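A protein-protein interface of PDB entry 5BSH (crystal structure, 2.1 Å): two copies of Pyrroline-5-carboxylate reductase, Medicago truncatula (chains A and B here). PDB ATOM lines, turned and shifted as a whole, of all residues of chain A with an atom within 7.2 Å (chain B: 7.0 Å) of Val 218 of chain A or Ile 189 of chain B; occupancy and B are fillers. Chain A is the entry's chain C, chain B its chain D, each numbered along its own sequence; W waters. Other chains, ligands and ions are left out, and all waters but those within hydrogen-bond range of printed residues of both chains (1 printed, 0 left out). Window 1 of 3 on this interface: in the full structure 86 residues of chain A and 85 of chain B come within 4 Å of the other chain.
O of Leu 213 of chain A lies within hydrogen-bond range of OG1 of Thr 217 of chain A (2.6 Å). The side-chain amide oxygen (OD1) of Asn 131 of chain B is in hydrogen-bond range of the backbone NH (N) of Ala 140 of chain B (3.1 Å). The side-chain hydroxyl (OG) of Ser 223 of chain B is in hydrogen-bond range of the backbone carbonyl oxygen (O) of Leu 219 of chain B (2.9 Å).
Among the printed residues, merely in contact across the chains: Ile 189 of chain A with Val 218 of chain B (3.8 Å), Ile 189 of chain A with Ala 221 of chain B (3.7 Å), Ala 192 of chain A with Leu 262 of chain B (3.6 Å), Leu 196 of chain A with Tyr 188 of chain B (3.9 Å), Ser 215 of chain A with Ala 222 of chain B (3.8 Å), Gln 216 of chain A with Ala 140 of chain B (3.7 Å), Thr 217 of chain A with Ala 140 of chain B (3.9 Å), Thr 217 of chain A with Gly 185 of chain B (3.8 Å), Thr 217 of chain A with Pro 186 of chain B (3.6 Å), Val 218 of chain A with Ile 189 of chain B (3.8 Å), Val 218 of chain A with Val 218 of chain B (3.5 Å), Val 218 of chain A with Ala 222 of chain B (3.7 Å), Leu 219 of chain A with Leu 219 of chain B (3.0 Å), Leu 219 of chain A with Ala 222 of chain B (3.4 Å), Leu 219 of chain A with Ser 223 of chain B (3.9 Å), Ala 221 of chain A with Pro 186 of chain B (3.9 Å), Ala 221 of chain A with Ile 189 of chain B (3.7 Å), Ala 221 of chain A with Tyr 190 of chain B (3.3 Å), Ala 222 of chain A with Val 218 of chain B (3.7 Å), Ala 222 of chain A with Leu 219 of chain B (3.4 Å), Ser 223 of chain A with Leu 219 of chain B (3.97 Å), Met 224 of chain A with Tyr 190 of chain B (3.4 Å), Ala 225 of chain A with Ile 193 of chain B (3.8 Å), Pro 232 of chain A with Tyr 190 of chain B (3.6 Å), Pro 232 of chain A with Glu 194 of chain B (3.9 Å), Leu 253 of chain A with Tyr 188 of chain B (3.7 Å), Phe 258 of chain A with Tyr 188 of chain B (3.6 Å), Phe 258 of chain A with Ala 192 of chain B (3.9 Å), Phe 258 of chain A with Leu 262 of chain B (3.9 Å), Leu 262 of chain A with Ala 192 of chain B (3.7 Å) and Leu 262 of chain A with Ala 195 of chain B (3.99 Å).
Leu 213 of chain A touches none of the printed residues of chain B. Of the printed residues of chain B, Leu 253 of chain A touches Tyr 188 (3.7 Å). Of the printed residues of chain A, Gly 185 of chain B touches Thr 217. Of chain A, only Val 218 and Ala 221 come within 4 Å of Ile 189 of chain B. Of the printed residues of chain A, Ala 221 of chain B touches Ile 189 (3.7 Å). The nearest printed residue of chain A that does not touch Val 218 of chain B is Leu 219 of chain A (5.5 Å).
Of the 22 printed residues of chain A, 17 touch a printed residue of chain B. Hydrophobic or aromatic side chains of chain A within 4 Å of the printed part of chain B: Ile 189, Ala 192, Leu 196, Val 218, Leu 219, Ala 221, Ala 222, Met 224, Ala 225, Pro 232, Leu 253, Phe 258 and Leu 262. Among the printed residues, 31 pairs touch across the chains. Among the printed residues, no Asp or Glu carboxylate lies within 4 Å of a Lys or Arg side-chain nitrogen of the other chain.
Ile 189 of chain A touches Ala 221 of chain B, and with the chains exchanged Ala 221 of chain A touches Ile 189 of chain B. Val 218 of chain A touches Ala 222 of chain B, and with the chains exchanged Ala 222 of chain A touches Val 218 of chain B.
Water W1 lies within hydrogen-bond range of the side-chain amide nitrogen of Asn 131 of chain B (2.9 Å), the backbone carbonyl oxygen of Gln 216 of chain A (2.9 Å) and the backbone NH of Ala 140 of chain B (3.2 Å).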
ATOM      1  N   ILE A 189     -26.669  26.298 -22.947  1.00  0.00           N
ATOM      2  CA  ILE A 189     -26.059  25.794 -24.181  1.00  0.00           C
ATOM      3  C   ILE A 189     -24.985  26.653 -24.763  1.00  0.00           C
ATOM      4  O   ILE A 189     -24.046  26.172 -25.317  1.00  0.00           O
ATOM      5  CB  ILE A 189     -27.165  25.464 -25.196  1.00  0.00           C
ATOM      6  CG1 ILE A 189     -28.142  24.464 -24.585  1.00  0.00           C
ATOM      7  CG2 ILE A 189     -26.556  24.900 -26.423  1.00  0.00           C
ATOM      8  CD1 ILE A 189     -27.506  23.165 -24.067  1.00  0.00           C
ATOM      9  N   ALA A 192     -22.099  25.758 -22.841  1.00  0.00           N
ATOM     10  CA  ALA A 192     -21.607  24.449 -23.334  1.00  0.00           C
ATOM     11  C   ALA A 192     -20.799  24.569 -24.599  1.00  0.00           C
ATOM     12  O   ALA A 192     -19.816  23.889 -24.798  1.00  0.00           O
ATOM     13  CB  ALA A 192     -22.771  23.507 -23.567  1.00  0.00           C
ATOM     14  N   ILE A 193     -21.306  25.358 -25.523  1.00  0.00           N
ATOM     15  CA  ILE A 193     -20.618  25.521 -26.816  1.00  0.00           C
ATOM     16  C   ILE A 193     -19.238  26.141 -26.641  1.00  0.00           C
ATOM     17  O   ILE A 193     -18.272  25.720 -27.230  1.00  0.00           O
ATOM     18  CB  ILE A 193     -21.470  26.421 -27.778  1.00  0.00           C
ATOM     19  CG1 ILE A 193     -22.657  25.582 -28.304  1.00  0.00           C
ATOM     20  CG2 ILE A 193     -20.623  26.930 -28.928  1.00  0.00           C
ATOM     21  CD1 ILE A 193     -23.716  26.340 -29.026  1.00  0.00           C
ATOM     22  N   LEU A 196     -17.021  23.501 -25.031  1.00  0.00           N
ATOM     23  CA  LEU A 196     -16.583  22.492 -26.015  1.00  0.00           C
ATOM     24  C   LEU A 196     -15.475  23.024 -26.962  1.00  0.00           C
ATOM     25  O   LEU A 196     -14.498  22.367 -27.220  1.00  0.00           O
ATOM     26  CB  LEU A 196     -17.769  22.048 -26.858  1.00  0.00           C
ATOM     27  CG  LEU A 196     -18.756  21.162 -26.130  1.00  0.00           C
ATOM     28  CD1 LEU A 196     -20.053  21.059 -26.884  1.00  0.00           C
ATOM     29  CD2 LEU A 196     -18.194  19.764 -25.914  1.00  0.00           C
ATOM     30  N   SER A 212     -16.475  26.536 -34.642  1.00  0.00           N
ATOM     31  CA  SER A 212     -17.352  26.058 -35.695  1.00  0.00           C
ATOM     32  C   SER A 212     -17.801  24.671 -35.455  1.00  0.00           C
ATOM     33  O   SER A 212     -18.969  24.341 -35.618  1.00  0.00           O
ATOM     34  CB  SER A 212     -16.646  26.129 -37.099  1.00  0.00           C
ATOM     35  OG  SER A 212     -16.258  27.444 -37.358  1.00  0.00           O
ATOM     36  N   LEU A 213     -16.873  23.779 -35.099  1.00  0.00           N
ATOM     37  CA  LEU A 213     -17.273  22.386 -34.825  1.00  0.00           C
ATOM     38  C   LEU A 213     -18.186  22.224 -33.628  1.00  0.00           C
ATOM     39  O   LEU A 213     -19.153  21.429 -33.656  1.00  0.00           O
ATOM     40  CB  LEU A 213     -16.070  21.470 -34.668  1.00  0.00           C
ATOM     41  CG  LEU A 213     -15.194  21.233 -35.898  1.00  0.00           C
ATOM     42  CD1 LEU A 213     -13.962  20.410 -35.533  1.00  0.00           C
ATOM     43  CD2 LEU A 213     -15.955  20.519 -36.993  1.00  0.00           C
ATOM     44  N   ALA A 214     -17.924  22.995 -32.570  1.00  0.00           N
ATOM     45  CA  ALA A 214     -18.725  22.904 -31.334  1.00  0.00           C
ATOM     46  C   ALA A 214     -20.179  23.280 -31.630  1.00  0.00           C
ATOM     47  O   ALA A 214     -21.112  22.524 -31.356  1.00  0.00           O
ATOM     48  CB  ALA A 214     -18.150  23.839 -30.307  1.00  0.00           C
ATOM     49  N   SER A 215     -20.357  24.421 -32.311  1.00  0.00           N
ATOM     50  CA  SER A 215     -21.724  24.858 -32.665  1.00  0.00           C
ATOM     51  C   SER A 215     -22.460  23.896 -33.533  1.00  0.00           C
ATOM     52  O   SER A 215     -23.607  23.516 -33.254  1.00  0.00           O
ATOM     53  CB  SER A 215     -21.717  26.233 -33.329  1.00  0.00           C
ATOM     54  OG  SER A 215     -21.180  27.172 -32.406  1.00  0.00           O
ATOM     55  N   GLN A 216     -21.811  23.413 -34.549  1.00  0.00           N
ATOM     56  CA  GLN A 216     -22.504  22.504 -35.465  1.00  0.00           C
ATOM     57  C   GLN A 216     -22.727  21.131 -34.888  1.00  0.00           C
ATOM     58  O   GLN A 216     -23.695  20.438 -35.207  1.00  0.00           O
ATOM     59  CB  GLN A 216     -21.675  22.347 -36.757  1.00  0.00           C
ATOM     60  CG  GLN A 216     -22.303  21.436 -37.796  1.00  0.00           C
ATOM     61  CD  GLN A 216     -23.627  21.986 -38.362  1.00  0.00           C
ATOM     62  OE1 GLN A 216     -23.810  23.179 -38.422  1.00  0.00           O
ATOM     63  NE2 GLN A 216     -24.560  21.112 -38.642  1.00  0.00           N
ATOM     64  N   THR A 217     -21.806  20.695 -34.044  1.00  0.00           N
ATOM     65  CA  THR A 217     -22.000  19.439 -33.320  1.00  0.00           C
ATOM     66  C   THR A 217     -23.211  19.471 -32.420  1.00  0.00           C
ATOM     67  O   THR A 217     -24.035  18.547 -32.442  1.00  0.00           O
ATOM     68  CB  THR A 217     -20.758  19.108 -32.496  1.00  0.00           C
ATOM     69  OG1 THR A 217     -19.664  18.908 -33.396  1.00  0.00           O
ATOM     70  CG2 THR A 217     -20.947  17.874 -31.654  1.00  0.00           C
ATOM     71  N   VAL A 218     -23.370  20.572 -31.673  1.00  0.00           N
ATOM     72  CA  VAL A 218     -24.555  20.752 -30.869  1.00  0.00           C
ATOM     73  C   VAL A 218     -25.826  20.839 -31.723  1.00  0.00           C
ATOM     74  O   VAL A 218     -26.852  20.209 -31.415  1.00  0.00           O
ATOM     75  CB  VAL A 218     -24.465  22.000 -29.972  1.00  0.00           C
ATOM     76  CG1 VAL A 218     -25.748  22.147 -29.172  1.00  0.00           C
ATOM     77  CG2 VAL A 218     -23.300  21.877 -28.995  1.00  0.00           C
ATOM     78  N   LEU A 219     -25.764  21.630 -32.779  1.00  0.00           N
ATOM     79  CA  LEU A 219     -26.928  21.717 -33.740  1.00  0.00           C
ATOM     80  C   LEU A 219     -27.312  20.330 -34.316  1.00  0.00           C
ATOM     81  O   LEU A 219     -28.459  19.860 -34.248  1.00  0.00           O
ATOM     82  CB  LEU A 219     -26.628  22.689 -34.868  1.00  0.00           C
ATOM     83  CG  LEU A 219     -27.607  22.742 -36.065  1.00  0.00           C
ATOM     84  CD1 LEU A 219     -28.988  22.826 -35.576  1.00  0.00           C
ATOM     85  CD2 LEU A 219     -27.355  24.003 -36.887  1.00  0.00           C
ATOM     86  N   GLY A 220     -26.324  19.630 -34.818  1.00  0.00           N
ATOM     87  CA  GLY A 220     -26.554  18.258 -35.317  1.00  0.00           C
ATOM     88  C   GLY A 220     -27.167  17.288 -34.318  1.00  0.00           C
ATOM     89  O   GLY A 220     -28.091  16.537 -34.599  1.00  0.00           O
ATOM     90  N   ALA A 221     -26.636  17.270 -33.127  1.00  0.00           N
ATOM     91  CA  ALA A 221     -27.158  16.357 -32.103  1.00  0.00           C
ATOM     92  C   ALA A 221     -28.595  16.632 -31.765  1.00  0.00           C
ATOM     93  O   ALA A 221     -29.398  15.710 -31.597  1.00  0.00           O
ATOM     94  CB  ALA A 221     -26.294  16.448 -30.829  1.00  0.00           C
ATOM     95  N   ALA A 222     -28.914  17.900 -31.565  1.00  0.00           N
ATOM     96  CA  ALA A 222     -30.249  18.274 -31.242  1.00  0.00           C
ATOM     97  C   ALA A 222     -31.200  17.952 -32.373  1.00  0.00           C
ATOM     98  O   ALA A 222     -32.349  17.578 -32.127  1.00  0.00           O
ATOM     99  CB  ALA A 222     -30.333  19.797 -30.951  1.00  0.00           C
ATOM    100  N   SER A 223     -30.754  18.144 -33.604  1.00  0.00           N
ATOM    101  CA  SER A 223     -31.574  17.723 -34.786  1.00  0.00           C
ATOM    102  C   SER A 223     -31.818  16.230 -34.783  1.00  0.00           C
ATOM    103  O   SER A 223     -32.895  15.784 -35.173  1.00  0.00           O
ATOM    104  CB  SER A 223     -30.876  18.051 -36.114  1.00  0.00           C
ATOM    105  OG  SER A 223     -30.580  19.403 -36.138  1.00  0.00           O
ATOM    106  N   MET A 224     -30.806  15.447 -34.423  1.00  0.00           N
ATOM    107  CA  MET A 224     -31.015  14.000 -34.290  1.00  0.00           C
ATOM    108  C   MET A 224     -32.077  13.744 -33.241  1.00  0.00           C
ATOM    109  O   MET A 224     -32.897  12.842 -33.373  1.00  0.00           O
ATOM    110  CB  MET A 224     -29.719  13.268 -33.929  1.00  0.00           C
ATOM    111  CG  MET A 224     -28.662  13.282 -35.022  1.00  0.00           C
ATOM    112  SD  MET A 224     -29.067  12.184 -36.394  1.00  0.00           S
ATOM    113  CE  MET A 224     -28.691  10.584 -35.675  1.00  0.00           C
ATOM    114  N   ALA A 225     -32.036  14.497 -32.133  1.00  0.00           N
ATOM    115  CA  ALA A 225     -32.970  14.243 -31.067  1.00  0.00           C
ATOM    116  C   ALA A 225     -34.388  14.615 -31.540  1.00  0.00           C
ATOM    117  O   ALA A 225     -35.360  13.994 -31.159  1.00  0.00           O
ATOM    118  CB  ALA A 225     -32.611  15.027 -29.847  1.00  0.00           C
ATOM    119  N   PRO A 232     -33.124   9.923 -25.773  1.00  0.00           N
ATOM    120  CA  PRO A 232     -31.734  10.399 -25.713  1.00  0.00           C
ATOM    121  C   PRO A 232     -30.745   9.371 -25.257  1.00  0.00           C
ATOM    122  O   PRO A 232     -29.633   9.318 -25.733  1.00  0.00           O
ATOM    123  CB  PRO A 232     -31.776  11.499 -24.640  1.00  0.00           C
ATOM    124  CG  PRO A 232     -33.177  11.953 -24.585  1.00  0.00           C
ATOM    125  CD  PRO A 232     -34.054  10.824 -25.055  1.00  0.00           C
ATOM    126  N   LEU A 253     -17.920  12.944 -18.099  1.00  0.00           N
ATOM    127  CA  LEU A 253     -19.093  13.701 -17.745  1.00  0.00           C
ATOM    128  C   LEU A 253     -19.781  13.088 -16.502  1.00  0.00           C
ATOM    129  O   LEU A 253     -20.199  13.804 -15.563  1.00  0.00           O
ATOM    130  CB  LEU A 253     -20.074  13.784 -18.891  1.00  0.00           C
ATOM    131  CG  LEU A 253     -19.573  14.469 -20.146  1.00  0.00           C
ATOM    132  CD1 LEU A 253     -20.696  14.405 -21.178  1.00  0.00           C
ATOM    133  CD2 LEU A 253     -19.206  15.919 -19.886  1.00  0.00           C
ATOM    134  N   PHE A 258     -22.378  15.638 -14.355  1.00  0.00           N
ATOM    135  CA  PHE A 258     -22.840  16.550 -15.403  1.00  0.00           C
ATOM    136  C   PHE A 258     -24.333  16.661 -15.488  1.00  0.00           C
ATOM    137  O   PHE A 258     -24.941  17.783 -15.547  1.00  0.00           O
ATOM    138  CB  PHE A 258     -22.246  16.056 -16.712  1.00  0.00           C
ATOM    139  CG  PHE A 258     -22.633  16.842 -17.955  1.00  0.00           C
ATOM    140  CD1 PHE A 258     -22.083  18.065 -18.251  1.00  0.00           C
ATOM    141  CD2 PHE A 258     -23.477  16.263 -18.902  1.00  0.00           C
ATOM    142  CE1 PHE A 258     -22.438  18.741 -19.443  1.00  0.00           C
ATOM    143  CE2 PHE A 258     -23.806  16.872 -20.112  1.00  0.00           C
ATOM    144  CZ  PHE A 258     -23.209  18.094 -20.435  1.00  0.00           C
ATOM    145  N   LEU A 262     -26.973  20.137 -14.686  1.00  0.00           N
ATOM    146  CA  LEU A 262     -27.958  20.733 -15.597  1.00  0.00           C
ATOM    147  C   LEU A 262     -29.357  20.650 -14.968  1.00  0.00           C
ATOM    148  O   LEU A 262     -30.165  21.589 -15.053  1.00  0.00           O
ATOM    149  CB  LEU A 262     -27.906  20.038 -16.916  1.00  0.00           C
ATOM    150  CG  LEU A 262     -26.811  20.497 -17.843  1.00  0.00           C
ATOM    151  CD1 LEU A 262     -26.670  19.484 -18.939  1.00  0.00           C
ATOM    152  CD2 LEU A 262     -27.169  21.787 -18.486  1.00  0.00           C
ATOM    153  N   ASN B 131     -19.662  13.078 -38.793  1.00  0.00           N
ATOM    154  CA  ASN B 131     -20.210  12.585 -37.524  1.00  0.00           C
ATOM    155  C   ASN B 131     -21.595  12.069 -37.731  1.00  0.00           C
ATOM    156  O   ASN B 131     -22.150  12.142 -38.818  1.00  0.00           O
ATOM    157  CB  ASN B 131     -20.078  13.679 -36.391  1.00  0.00           C
ATOM    158  CG  ASN B 131     -21.075  14.820 -36.523  1.00  0.00           C
ATOM    159  OD1 ASN B 131     -21.921  14.855 -37.448  1.00  0.00           O
ATOM    160  ND2 ASN B 131     -21.013  15.758 -35.565  1.00  0.00           N
ATOM    161  N   ALA B 140     -21.211  17.535 -38.810  1.00  0.00           N
ATOM    162  CA  ALA B 140     -20.000  18.374 -38.690  1.00  0.00           C
ATOM    163  C   ALA B 140     -18.829  17.555 -39.203  1.00  0.00           C
ATOM    164  O   ALA B 140     -18.497  16.522 -38.645  1.00  0.00           O
ATOM    165  CB  ALA B 140     -19.757  18.828 -37.283  1.00  0.00           C
ATOM    166  N   SER B 184     -17.387  12.743 -30.961  1.00  0.00           N
ATOM    167  CA  SER B 184     -17.889  12.266 -29.711  1.00  0.00           C
ATOM    168  C   SER B 184     -18.870  13.211 -29.108  1.00  0.00           C
ATOM    169  O   SER B 184     -19.701  12.808 -28.317  1.00  0.00           O
ATOM    170  CB  SER B 184     -16.735  12.039 -28.761  1.00  0.00           C
ATOM    171  OG  SER B 184     -15.860  11.080 -29.305  1.00  0.00           O
ATOM    172  N   GLY B 185     -18.800  14.476 -29.491  1.00  0.00           N
ATOM    173  CA  GLY B 185     -19.646  15.524 -28.894  1.00  0.00           C
ATOM    174  C   GLY B 185     -21.134  15.247 -28.905  1.00  0.00           C
ATOM    175  O   GLY B 185     -21.835  15.627 -27.983  1.00  0.00           O
ATOM    176  N   PRO B 186     -21.646  14.508 -29.898  1.00  0.00           N
ATOM    177  CA  PRO B 186     -23.102  14.350 -29.863  1.00  0.00           C
ATOM    178  C   PRO B 186     -23.598  13.640 -28.616  1.00  0.00           C
ATOM    179  O   PRO B 186     -24.644  13.942 -28.103  1.00  0.00           O
ATOM    180  CB  PRO B 186     -23.384  13.530 -31.139  1.00  0.00           C
ATOM    181  CG  PRO B 186     -22.357  14.024 -32.096  1.00  0.00           C
ATOM    182  CD  PRO B 186     -21.096  14.271 -31.240  1.00  0.00           C
ATOM    183  N   ALA B 187     -22.840  12.692 -28.127  1.00  0.00           N
ATOM    184  CA  ALA B 187     -23.232  12.017 -26.963  1.00  0.00           C
ATOM    185  C   ALA B 187     -23.311  12.944 -25.746  1.00  0.00           C
ATOM    186  O   ALA B 187     -24.160  12.748 -24.852  1.00  0.00           O
ATOM    187  CB  ALA B 187     -22.288  10.870 -26.681  1.00  0.00           C
ATOM    188  N   TYR B 188     -22.392  13.892 -25.671  1.00  0.00           N
ATOM    189  CA  TYR B 188     -22.385  14.836 -24.546  1.00  0.00           C
ATOM    190  C   TYR B 188     -23.651  15.628 -24.564  1.00  0.00           C
ATOM    191  O   TYR B 188     -24.282  15.880 -23.514  1.00  0.00           O
ATOM    192  CB  TYR B 188     -21.209  15.801 -24.541  1.00  0.00           C
ATOM    193  CG  TYR B 188     -19.817  15.200 -24.855  1.00  0.00           C
ATOM    194  CD1 TYR B 188     -19.544  13.857 -24.662  1.00  0.00           C
ATOM    195  CD2 TYR B 188     -18.831  15.991 -25.420  1.00  0.00           C
ATOM    196  CE1 TYR B 188     -18.301  13.329 -24.991  1.00  0.00           C
ATOM    197  CE2 TYR B 188     -17.594  15.511 -25.734  1.00  0.00           C
ATOM    198  CZ  TYR B 188     -17.324  14.142 -25.524  1.00  0.00           C
ATOM    199  OH  TYR B 188     -16.120  13.648 -25.918  1.00  0.00           O
ATOM    200  N   ILE B 189     -24.099  15.937 -25.762  1.00  0.00           N
ATOM    201  CA  ILE B 189     -25.368  16.655 -25.916  1.00  0.00           C
ATOM    202  C   ILE B 189     -26.620  15.813 -25.703  1.00  0.00           C
ATOM    203  O   ILE B 189     -27.609  16.315 -25.211  1.00  0.00           O
ATOM    204  CB  ILE B 189     -25.389  17.326 -27.298  1.00  0.00           C
ATOM    205  CG1 ILE B 189     -24.175  18.255 -27.396  1.00  0.00           C
ATOM    206  CG2 ILE B 189     -26.646  18.086 -27.476  1.00  0.00           C
ATOM    207  CD1 ILE B 189     -24.041  19.279 -26.266  1.00  0.00           C
ATOM    208  N   TYR B 190     -26.564  14.498 -25.993  1.00  0.00           N
ATOM    209  CA  TYR B 190     -27.664  13.619 -25.673  1.00  0.00           C
ATOM    210  C   TYR B 190     -27.830  13.562 -24.161  1.00  0.00           C
ATOM    211  O   TYR B 190     -28.945  13.561 -23.677  1.00  0.00           O
ATOM    212  CB  TYR B 190     -27.473  12.233 -26.314  1.00  0.00           C
ATOM    213  CG  TYR B 190     -27.379  12.233 -27.867  1.00  0.00           C
ATOM    214  CD1 TYR B 190     -28.104  13.150 -28.656  1.00  0.00           C
ATOM    215  CD2 TYR B 190     -26.609  11.285 -28.548  1.00  0.00           C
ATOM    216  CE1 TYR B 190     -28.006  13.153 -30.058  1.00  0.00           C
ATOM    217  CE2 TYR B 190     -26.505  11.279 -29.934  1.00  0.00           C
ATOM    218  CZ  TYR B 190     -27.207  12.237 -30.696  1.00  0.00           C
ATOM    219  OH  TYR B 190     -27.164  12.192 -32.044  1.00  0.00           O
ATOM    220  N   LEU B 191     -26.744  13.451 -23.398  1.00  0.00           N
ATOM    221  CA  LEU B 191     -26.831  13.479 -21.953  1.00  0.00           C
ATOM    222  C   LEU B 191     -27.433  14.823 -21.523  1.00  0.00           C
ATOM    223  O   LEU B 191     -28.288  14.876 -20.654  1.00  0.00           O
ATOM    224  CB  LEU B 191     -25.462  13.351 -21.288  1.00  0.00           C
ATOM    225  CG  LEU B 191     -25.087  11.933 -20.830  1.00  0.00           C
ATOM    226  CD1 LEU B 191     -25.024  10.993 -21.980  1.00  0.00           C
ATOM    227  CD2 LEU B 191     -23.785  11.923 -20.048  1.00  0.00           C
ATOM    228  N   ALA B 192     -26.972  15.889 -22.101  1.00  0.00           N
ATOM    229  CA  ALA B 192     -27.493  17.190 -21.707  1.00  0.00           C
ATOM    230  C   ALA B 192     -28.983  17.307 -21.941  1.00  0.00           C
ATOM    231  O   ALA B 192     -29.687  17.890 -21.132  1.00  0.00           O
ATOM    232  CB  ALA B 192     -26.814  18.301 -22.497  1.00  0.00           C
ATOM    233  N   ILE B 193     -29.434  16.846 -23.101  1.00  0.00           N
ATOM    234  CA  ILE B 193     -30.915  16.887 -23.420  1.00  0.00           C
ATOM    235  C   ILE B 193     -31.735  16.088 -22.424  1.00  0.00           C
ATOM    236  O   ILE B 193     -32.720  16.547 -21.903  1.00  0.00           O
ATOM    237  CB  ILE B 193     -31.184  16.405 -24.850  1.00  0.00           C
ATOM    238  CG1 ILE B 193     -30.702  17.470 -25.809  1.00  0.00           C
ATOM    239  CG2 ILE B 193     -32.651  16.100 -25.043  1.00  0.00           C
ATOM    240  CD1 ILE B 193     -30.633  17.021 -27.263  1.00  0.00           C
ATOM    241  N   GLU B 194     -31.227  14.925 -22.044  1.00  0.00           N
ATOM    242  CA  GLU B 194     -31.911  14.136 -21.097  1.00  0.00           C
ATOM    243  C   GLU B 194     -31.925  14.784 -19.742  1.00  0.00           C
ATOM    244  O   GLU B 194     -32.940  14.763 -19.014  1.00  0.00           O
ATOM    245  CB  GLU B 194     -31.288  12.684 -20.978  1.00  0.00           C
ATOM    246  CG  GLU B 194     -32.178  11.819 -20.090  1.00  0.00           C
ATOM    247  CD  GLU B 194     -31.778  10.362 -20.058  1.00  0.00           C
ATOM    248  OE1 GLU B 194     -30.643  10.020 -20.507  1.00  0.00           O
ATOM    249  OE2 GLU B 194     -32.636   9.562 -19.566  1.00  0.00           O
ATOM    250  N   ALA B 195     -30.792  15.313 -19.352  1.00  0.00           N
ATOM    251  CA  ALA B 195     -30.685  15.979 -18.025  1.00  0.00           C
ATOM    252  C   ALA B 195     -31.537  17.229 -17.971  1.00  0.00           C
ATOM    253  O   ALA B 195     -32.171  17.528 -16.977  1.00  0.00           O
ATOM    254  CB  ALA B 195     -29.214  16.359 -17.756  1.00  0.00           C
ATOM    255  N   LEU B 196     -31.579  17.965 -19.047  1.00  0.00           N
ATOM    256  CA  LEU B 196     -32.526  19.115 -19.076  1.00  0.00           C
ATOM    257  C   LEU B 196     -33.978  18.713 -18.932  1.00  0.00           C
ATOM    258  O   LEU B 196     -34.759  19.344 -18.215  1.00  0.00           O
ATOM    259  CB  LEU B 196     -32.365  19.914 -20.392  1.00  0.00           C
ATOM    260  CG  LEU B 196     -31.056  20.717 -20.453  1.00  0.00           C
ATOM    261  CD1 LEU B 196     -30.776  21.144 -21.873  1.00  0.00           C
ATOM    262  CD2 LEU B 196     -31.068  21.944 -19.547  1.00  0.00           C
ATOM    263  N   VAL B 218     -32.150  23.218 -27.140  1.00  0.00           N
ATOM    264  CA  VAL B 218     -30.794  23.000 -27.602  1.00  0.00           C
ATOM    265  C   VAL B 218     -30.627  23.322 -29.074  1.00  0.00           C
ATOM    266  O   VAL B 218     -29.621  23.944 -29.494  1.00  0.00           O
ATOM    267  CB  VAL B 218     -30.315  21.552 -27.322  1.00  0.00           C
ATOM    268  CG1 VAL B 218     -28.921  21.343 -27.841  1.00  0.00           C
ATOM    269  CG2 VAL B 218     -30.308  21.291 -25.802  1.00  0.00           C
ATOM    270  N   LEU B 219     -31.551  22.828 -29.888  1.00  0.00           N
ATOM    271  CA  LEU B 219     -31.503  23.130 -31.352  1.00  0.00           C
ATOM    272  C   LEU B 219     -31.520  24.624 -31.623  1.00  0.00           C
ATOM    273  O   LEU B 219     -30.673  25.188 -32.343  1.00  0.00           O
ATOM    274  CB  LEU B 219     -32.665  22.432 -32.067  1.00  0.00           C
ATOM    275  CG  LEU B 219     -32.923  22.813 -33.546  1.00  0.00           C
ATOM    276  CD1 LEU B 219     -31.656  22.746 -34.297  1.00  0.00           C
ATOM    277  CD2 LEU B 219     -33.844  21.752 -34.177  1.00  0.00           C
ATOM    278  N   ALA B 221     -30.728  27.197 -29.570  1.00  0.00           N
ATOM    279  CA  ALA B 221     -29.481  27.856 -29.112  1.00  0.00           C
ATOM    280  C   ALA B 221     -28.301  27.670 -30.038  1.00  0.00           C
ATOM    281  O   ALA B 221     -27.582  28.600 -30.341  1.00  0.00           O
ATOM    282  CB  ALA B 221     -29.111  27.301 -27.718  1.00  0.00           C
ATOM    283  N   ALA B 222     -28.124  26.435 -30.525  1.00  0.00           N
ATOM    284  CA  ALA B 222     -27.064  26.118 -31.487  1.00  0.00           C
ATOM    285  C   ALA B 222     -27.255  26.801 -32.792  1.00  0.00           C
ATOM    286  O   ALA B 222     -26.287  27.292 -33.411  1.00  0.00           O
ATOM    287  CB  ALA B 222     -26.952  24.614 -31.724  1.00  0.00           C
ATOM    288  N   SER B 223     -28.497  26.929 -33.201  1.00  0.00           N
ATOM    289  CA  SER B 223     -28.793  27.733 -34.438  1.00  0.00           C
ATOM    290  C   SER B 223     -28.488  29.167 -34.281  1.00  0.00           C
ATOM    291  O   SER B 223     -28.016  29.828 -35.232  1.00  0.00           O
ATOM    292  CB  SER B 223     -30.248  27.651 -34.807  1.00  0.00           C
ATOM    293  OG  SER B 223     -30.620  26.319 -34.979  1.00  0.00           O
ATOM    294  N   LEU B 262     -16.984  19.836 -19.412  1.00  0.00           N
ATOM    295  CA  LEU B 262     -17.068  19.609 -20.865  1.00  0.00           C
ATOM    296  C   LEU B 262     -15.694  19.664 -21.510  1.00  0.00           C
ATOM    297  O   LEU B 262     -15.352  18.877 -22.416  1.00  0.00           O
ATOM    298  CB  LEU B 262     -17.985  20.622 -21.524  1.00  0.00           C
ATOM    299  CG  LEU B 262     -19.438  20.298 -21.350  1.00  0.00           C
ATOM    300  CD1 LEU B 262     -20.266  21.517 -21.652  1.00  0.00           C
ATOM    301  CD2 LEU B 262     -19.881  19.205 -22.299  1.00  0.00           C
HETATM  302  O   HOH W   1     -23.066  17.715 -36.151  1.00  0.00           O
